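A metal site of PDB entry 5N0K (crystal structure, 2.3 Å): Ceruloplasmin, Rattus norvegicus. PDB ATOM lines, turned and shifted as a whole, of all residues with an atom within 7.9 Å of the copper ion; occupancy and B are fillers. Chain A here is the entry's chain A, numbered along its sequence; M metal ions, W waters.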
ATOM      1  N   LEU A 297     -36.250 -10.083   6.918  1.00  0.00           N
ATOM      2  CA  LEU A 297     -34.958  -9.741   7.470  1.00  0.00           C
ATOM      3  C   LEU A 297     -35.140  -9.153   8.857  1.00  0.00           C
ATOM      4  O   LEU A 297     -35.861  -8.176   9.036  1.00  0.00           O
ATOM      5  CB  LEU A 297     -34.335  -8.689   6.578  1.00  0.00           C
ATOM      6  CG  LEU A 297     -32.826  -8.550   6.398  1.00  0.00           C
ATOM      7  CD1 LEU A 297     -32.391  -7.109   6.092  1.00  0.00           C
ATOM      8  CD2 LEU A 297     -31.986  -9.177   7.481  1.00  0.00           C
ATOM      9  N   GLN A 301     -29.582  -8.642  13.509  1.00  0.00           N
ATOM     10  CA  GLN A 301     -29.581  -9.836  14.359  1.00  0.00           C
ATOM     11  C   GLN A 301     -28.969 -11.045  13.702  1.00  0.00           C
ATOM     12  O   GLN A 301     -28.670 -11.050  12.515  1.00  0.00           O
ATOM     13  CB  GLN A 301     -30.983 -10.138  14.841  1.00  0.00           C
ATOM     14  CG  GLN A 301     -31.652  -8.972  15.598  1.00  0.00           C
ATOM     15  CD  GLN A 301     -30.945  -8.595  16.880  1.00  0.00           C
ATOM     16  OE1 GLN A 301     -30.606  -9.458  17.665  1.00  0.00           O
ATOM     17  NE2 GLN A 301     -30.735  -7.294  17.103  1.00  0.00           N
ATOM     18  N   ALA A 302     -28.736 -12.068  14.519  1.00  0.00           N
ATOM     19  CA  ALA A 302     -28.099 -13.285  14.067  1.00  0.00           C
ATOM     20  C   ALA A 302     -29.035 -14.470  14.290  1.00  0.00           C
ATOM     21  O   ALA A 302     -29.386 -14.783  15.437  1.00  0.00           O
ATOM     22  CB  ALA A 302     -26.773 -13.479  14.762  1.00  0.00           C
ATOM     23  N   LEU A 303     -29.445 -15.116  13.195  1.00  0.00           N
ATOM     24  CA  LEU A 303     -30.476 -16.143  13.237  1.00  0.00           C
ATOM     25  C   LEU A 303     -29.952 -17.531  12.843  1.00  0.00           C
ATOM     26  O   LEU A 303     -29.076 -17.673  11.975  1.00  0.00           O
ATOM     27  CB  LEU A 303     -31.640 -15.750  12.306  1.00  0.00           C
ATOM     28  CG  LEU A 303     -32.634 -14.637  12.636  1.00  0.00           C
ATOM     29  CD1 LEU A 303     -33.554 -14.987  13.797  1.00  0.00           C
ATOM     30  CD2 LEU A 303     -31.956 -13.343  12.992  1.00  0.00           C
ATOM     31  N   HIS A 309     -26.944 -21.362   9.775  1.00  0.00           N
ATOM     32  CA  HIS A 309     -27.085 -19.911   9.813  1.00  0.00           C
ATOM     33  C   HIS A 309     -28.112 -19.445   8.761  1.00  0.00           C
ATOM     34  O   HIS A 309     -28.121 -19.954   7.706  1.00  0.00           O
ATOM     35  CB  HIS A 309     -25.759 -19.268   9.551  1.00  0.00           C
ATOM     36  CG  HIS A 309     -25.834 -17.800   9.644  1.00  0.00           C
ATOM     37  ND1 HIS A 309     -25.986 -17.145  10.844  1.00  0.00           N
ATOM     38  CD2 HIS A 309     -25.910 -16.861   8.676  1.00  0.00           C
ATOM     39  CE1 HIS A 309     -26.112 -15.855  10.623  1.00  0.00           C
ATOM     40  NE2 HIS A 309     -26.043 -15.654   9.323  1.00  0.00           N
ATOM     41  N   THR A 310     -28.990 -18.533   9.108  1.00  0.00           N
ATOM     42  CA  THR A 310     -29.922 -17.930   8.145  1.00  0.00           C
ATOM     43  C   THR A 310     -29.796 -16.423   8.228  1.00  0.00           C
ATOM     44  O   THR A 310     -29.767 -15.835   9.321  1.00  0.00           O
ATOM     45  CB  THR A 310     -31.435 -18.135   8.476  1.00  0.00           C
ATOM     46  OG1 THR A 310     -31.671 -19.363   9.195  1.00  0.00           O
ATOM     47  CG2 THR A 310     -32.185 -18.132   7.211  1.00  0.00           C
ATOM     48  N   ASP A 311     -29.808 -15.797   7.061  1.00  0.00           N
ATOM     49  CA  ASP A 311     -29.830 -14.361   6.925  1.00  0.00           C
ATOM     50  C   ASP A 311     -31.180 -13.826   6.478  1.00  0.00           C
ATOM     51  O   ASP A 311     -31.537 -12.717   6.833  1.00  0.00           O
ATOM     52  CB  ASP A 311     -28.752 -13.958   5.942  1.00  0.00           C
ATOM     53  CG  ASP A 311     -27.399 -14.010   6.569  1.00  0.00           C
ATOM     54  OD1 ASP A 311     -26.526 -14.788   6.139  1.00  0.00           O
ATOM     55  OD2 ASP A 311     -27.237 -13.257   7.535  1.00  0.00           O
ATOM     56  N   ILE A 312     -31.919 -14.571   5.671  1.00  0.00           N
ATOM     57  CA  ILE A 312     -33.219 -14.158   5.247  1.00  0.00           C
ATOM     58  C   ILE A 312     -34.124 -15.332   5.464  1.00  0.00           C
ATOM     59  O   ILE A 312     -33.696 -16.447   5.252  1.00  0.00           O
ATOM     60  CB  ILE A 312     -33.187 -13.770   3.767  1.00  0.00           C
ATOM     61  CG1 ILE A 312     -34.291 -12.782   3.462  1.00  0.00           C
ATOM     62  CG2 ILE A 312     -33.300 -14.974   2.812  1.00  0.00           C
ATOM     63  CD1 ILE A 312     -33.871 -11.358   3.834  1.00  0.00           C
ATOM     64  N   MET A 477     -25.662  -7.196   4.574  1.00  0.00           N
ATOM     65  CA  MET A 477     -26.561  -8.166   5.189  1.00  0.00           C
ATOM     66  C   MET A 477     -25.710  -9.217   5.856  1.00  0.00           C
ATOM     67  O   MET A 477     -24.972  -9.905   5.172  1.00  0.00           O
ATOM     68  CB  MET A 477     -27.423  -8.800   4.111  1.00  0.00           C
ATOM     69  CG  MET A 477     -28.454  -9.805   4.616  1.00  0.00           C
ATOM     70  SD  MET A 477     -29.198 -10.770   3.272  1.00  0.00           S
ATOM     71  CE  MET A 477     -27.850 -11.892   2.854  1.00  0.00           C
ATOM     72  N   GLY A 478     -25.785  -9.328   7.187  1.00  0.00           N
ATOM     73  CA  GLY A 478     -25.170 -10.449   7.884  1.00  0.00           C
ATOM     74  C   GLY A 478     -23.818 -10.212   8.559  1.00  0.00           C
ATOM     75  O   GLY A 478     -23.031 -11.154   8.736  1.00  0.00           O
ATOM     76  N   VAL A 479     -23.533  -8.967   8.931  1.00  0.00           N
ATOM     77  CA  VAL A 479     -22.422  -8.658   9.829  1.00  0.00           C
ATOM     78  C   VAL A 479     -22.965  -7.683  10.840  1.00  0.00           C
ATOM     79  O   VAL A 479     -24.073  -7.222  10.712  1.00  0.00           O
ATOM     80  CB  VAL A 479     -21.155  -8.116   9.100  1.00  0.00           C
ATOM     81  CG1 VAL A 479     -20.504  -9.197   8.254  1.00  0.00           C
ATOM     82  CG2 VAL A 479     -21.483  -6.910   8.243  1.00  0.00           C
ATOM     83  N   ARG A 480     -22.170  -7.427  11.871  1.00  0.00           N
ATOM     84  CA  ARG A 480     -22.588  -6.629  13.034  1.00  0.00           C
ATOM     85  C   ARG A 480     -22.064  -5.215  12.884  1.00  0.00           C
ATOM     86  O   ARG A 480     -20.890  -4.992  12.645  1.00  0.00           O
ATOM     87  CB  ARG A 480     -22.129  -7.313  14.334  1.00  0.00           C
ATOM     88  CG  ARG A 480     -21.756  -6.471  15.552  1.00  0.00           C
ATOM     89  CD  ARG A 480     -22.928  -5.934  16.317  1.00  0.00           C
ATOM     90  NE  ARG A 480     -22.785  -6.072  17.788  1.00  0.00           N
ATOM     91  CZ  ARG A 480     -23.009  -7.198  18.470  1.00  0.00           C
ATOM     92  NH1 ARG A 480     -23.370  -8.343  17.867  1.00  0.00           N
ATOM     93  NH2 ARG A 480     -22.891  -7.180  19.799  1.00  0.00           N
ATOM     94  N   GLU A 518     -21.707 -15.667  16.028  1.00  0.00           N
ATOM     95  CA  GLU A 518     -23.142 -15.950  15.791  1.00  0.00           C
ATOM     96  C   GLU A 518     -23.533 -15.562  14.359  1.00  0.00           C
ATOM     97  O   GLU A 518     -24.498 -16.076  13.807  1.00  0.00           O
ATOM     98  CB  GLU A 518     -24.103 -15.356  16.865  1.00  0.00           C
ATOM     99  CG  GLU A 518     -23.629 -14.138  17.647  1.00  0.00           C
ATOM    100  CD  GLU A 518     -22.547 -14.445  18.698  1.00  0.00           C
ATOM    101  OE1 GLU A 518     -22.585 -15.502  19.403  1.00  0.00           O
ATOM    102  OE2 GLU A 518     -21.633 -13.623  18.807  1.00  0.00           O
ATOM    103  N   MET A 519     -22.750 -14.673  13.761  1.00  0.00           N
ATOM    104  CA  MET A 519     -22.962 -14.249  12.400  1.00  0.00           C
ATOM    105  C   MET A 519     -22.221 -15.104  11.395  1.00  0.00           C
ATOM    106  O   MET A 519     -22.434 -14.966  10.185  1.00  0.00           O
ATOM    107  CB  MET A 519     -22.637 -12.745  12.287  1.00  0.00           C
ATOM    108  CG  MET A 519     -23.920 -11.917  12.286  1.00  0.00           C
ATOM    109  SD  MET A 519     -23.836 -10.371  13.180  1.00  0.00           S
ATOM    110  CE  MET A 519     -25.548  -9.887  13.307  1.00  0.00           C
ATOM    111  N   GLY A 520     -21.362 -15.998  11.880  1.00  0.00           N
ATOM    112  CA  GLY A 520     -20.622 -16.899  11.013  1.00  0.00           C
ATOM    113  C   GLY A 520     -21.287 -18.249  10.820  1.00  0.00           C
ATOM    114  O   GLY A 520     -22.339 -18.516  11.390  1.00  0.00           O
ATOM    115  N   PRO A 521     -20.669 -19.123  10.023  1.00  0.00           N
ATOM    116  CA  PRO A 521     -21.172 -20.483   9.829  1.00  0.00           C
ATOM    117  C   PRO A 521     -21.311 -21.213  11.113  1.00  0.00           C
ATOM    118  O   PRO A 521     -20.468 -21.050  11.963  1.00  0.00           O
ATOM    119  CB  PRO A 521     -20.074 -21.179   9.030  1.00  0.00           C
ATOM    120  CG  PRO A 521     -19.275 -20.080   8.466  1.00  0.00           C
ATOM    121  CD  PRO A 521     -19.361 -18.935   9.394  1.00  0.00           C
ATOM    122  N   LEU A 529     -19.992 -18.715   4.064  1.00  0.00           N
ATOM    123  CA  LEU A 529     -21.374 -18.324   3.698  1.00  0.00           C
ATOM    124  C   LEU A 529     -21.371 -17.204   2.693  1.00  0.00           C
ATOM    125  O   LEU A 529     -20.587 -16.291   2.799  1.00  0.00           O
ATOM    126  CB  LEU A 529     -22.140 -17.816   4.910  1.00  0.00           C
ATOM    127  CG  LEU A 529     -22.240 -18.782   6.093  1.00  0.00           C
ATOM    128  CD1 LEU A 529     -22.640 -17.998   7.348  1.00  0.00           C
ATOM    129  CD2 LEU A 529     -23.207 -19.909   5.863  1.00  0.00           C
ATOM    130  N   SER A 530     -22.332 -17.234   1.801  1.00  0.00           N
ATOM    131  CA  SER A 530     -22.553 -16.194   0.806  1.00  0.00           C
ATOM    132  C   SER A 530     -23.454 -15.163   1.436  1.00  0.00           C
ATOM    133  O   SER A 530     -24.538 -15.496   1.907  1.00  0.00           O
ATOM    134  CB  SER A 530     -23.307 -16.793  -0.425  1.00  0.00           C
ATOM    135  OG  SER A 530     -23.950 -15.788  -1.214  1.00  0.00           O
ATOM    136  N   LYS A 531     -23.049 -13.912   1.394  1.00  0.00           N
ATOM    137  CA  LYS A 531     -23.966 -12.851   1.758  1.00  0.00           C
ATOM    138  C   LYS A 531     -23.810 -11.762   0.755  1.00  0.00           C
ATOM    139  O   LYS A 531     -23.302 -12.012  -0.355  1.00  0.00           O
ATOM    140  CB  LYS A 531     -23.672 -12.386   3.166  1.00  0.00           C
ATOM    141  CG  LYS A 531     -23.539 -13.555   4.126  1.00  0.00           C
ATOM    142  CD  LYS A 531     -23.801 -13.118   5.530  1.00  0.00           C
ATOM    143  CE  LYS A 531     -23.432 -14.246   6.460  1.00  0.00           C
ATOM    144  NZ  LYS A 531     -23.702 -13.777   7.812  1.00  0.00           N
ATOM    145  N   ILE A 553     -18.405 -14.739   4.275  1.00  0.00           N
ATOM    146  CA  ILE A 553     -18.077 -14.745   5.668  1.00  0.00           C
ATOM    147  C   ILE A 553     -17.702 -16.162   6.040  1.00  0.00           C
ATOM    148  O   ILE A 553     -18.497 -17.050   5.814  1.00  0.00           O
ATOM    149  CB  ILE A 553     -19.295 -14.310   6.514  1.00  0.00           C
ATOM    150  CG1 ILE A 553     -19.730 -12.902   6.119  1.00  0.00           C
ATOM    151  CG2 ILE A 553     -18.966 -14.400   8.006  1.00  0.00           C
ATOM    152  CD1 ILE A 553     -18.713 -11.829   6.456  1.00  0.00           C
ATOM    153  N   SER A 676     -29.397 -16.264  -0.329  1.00  0.00           N
ATOM    154  CA  SER A 676     -28.028 -16.586  -0.726  1.00  0.00           C
ATOM    155  C   SER A 676     -27.701 -18.044  -0.340  1.00  0.00           C
ATOM    156  O   SER A 676     -28.229 -18.548   0.613  1.00  0.00           O
ATOM    157  CB  SER A 676     -27.052 -15.605  -0.103  1.00  0.00           C
ATOM    158  OG  SER A 676     -27.261 -15.498   1.303  1.00  0.00           O
HETATM  159 CU    CU M   1     -25.774 -13.610   8.687  1.00  0.00          CU
HETATM  160  O   HOH W   1     -26.267 -12.268  10.539  1.00  0.00           O
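ND1 of His 309 sits at hydrogen-bond distance from O of Glu 518 (3.5 Å). ND1 of His 309 is in hydrogen-bond range of O of Leu 303 (3.3 Å). The backbone carbonyl oxygen (O) of Gly 478 lies close to the side-chain amino group (NZ) of Lys 531, at 2.9 Å. NZ of Lys 531 sits close to O of Met 519 (2.9 Å). The backbone NH of Arg 480 is in hydrogen-bond range of the side-chain sulfur of Met 519, 3.6 Å away.
Residues that only touch the copper ion: Gly 478 (3.3 Å) and Met 519 (3.9 Å). Five residues have an atom within 4 Å of the copper ion: His 309, Asp 311, Gly 478, Met 519 and Lys 531.
The copper ion is bound by the side-chain carboxylate (OD2) of Asp 311 (1.9 Å), a ring nitrogen (NE2) of His 309 (2.2 Å), the side-chain amino group (NZ) of Lys 531 (2.3 Å) and water W1 (2.3 Å).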
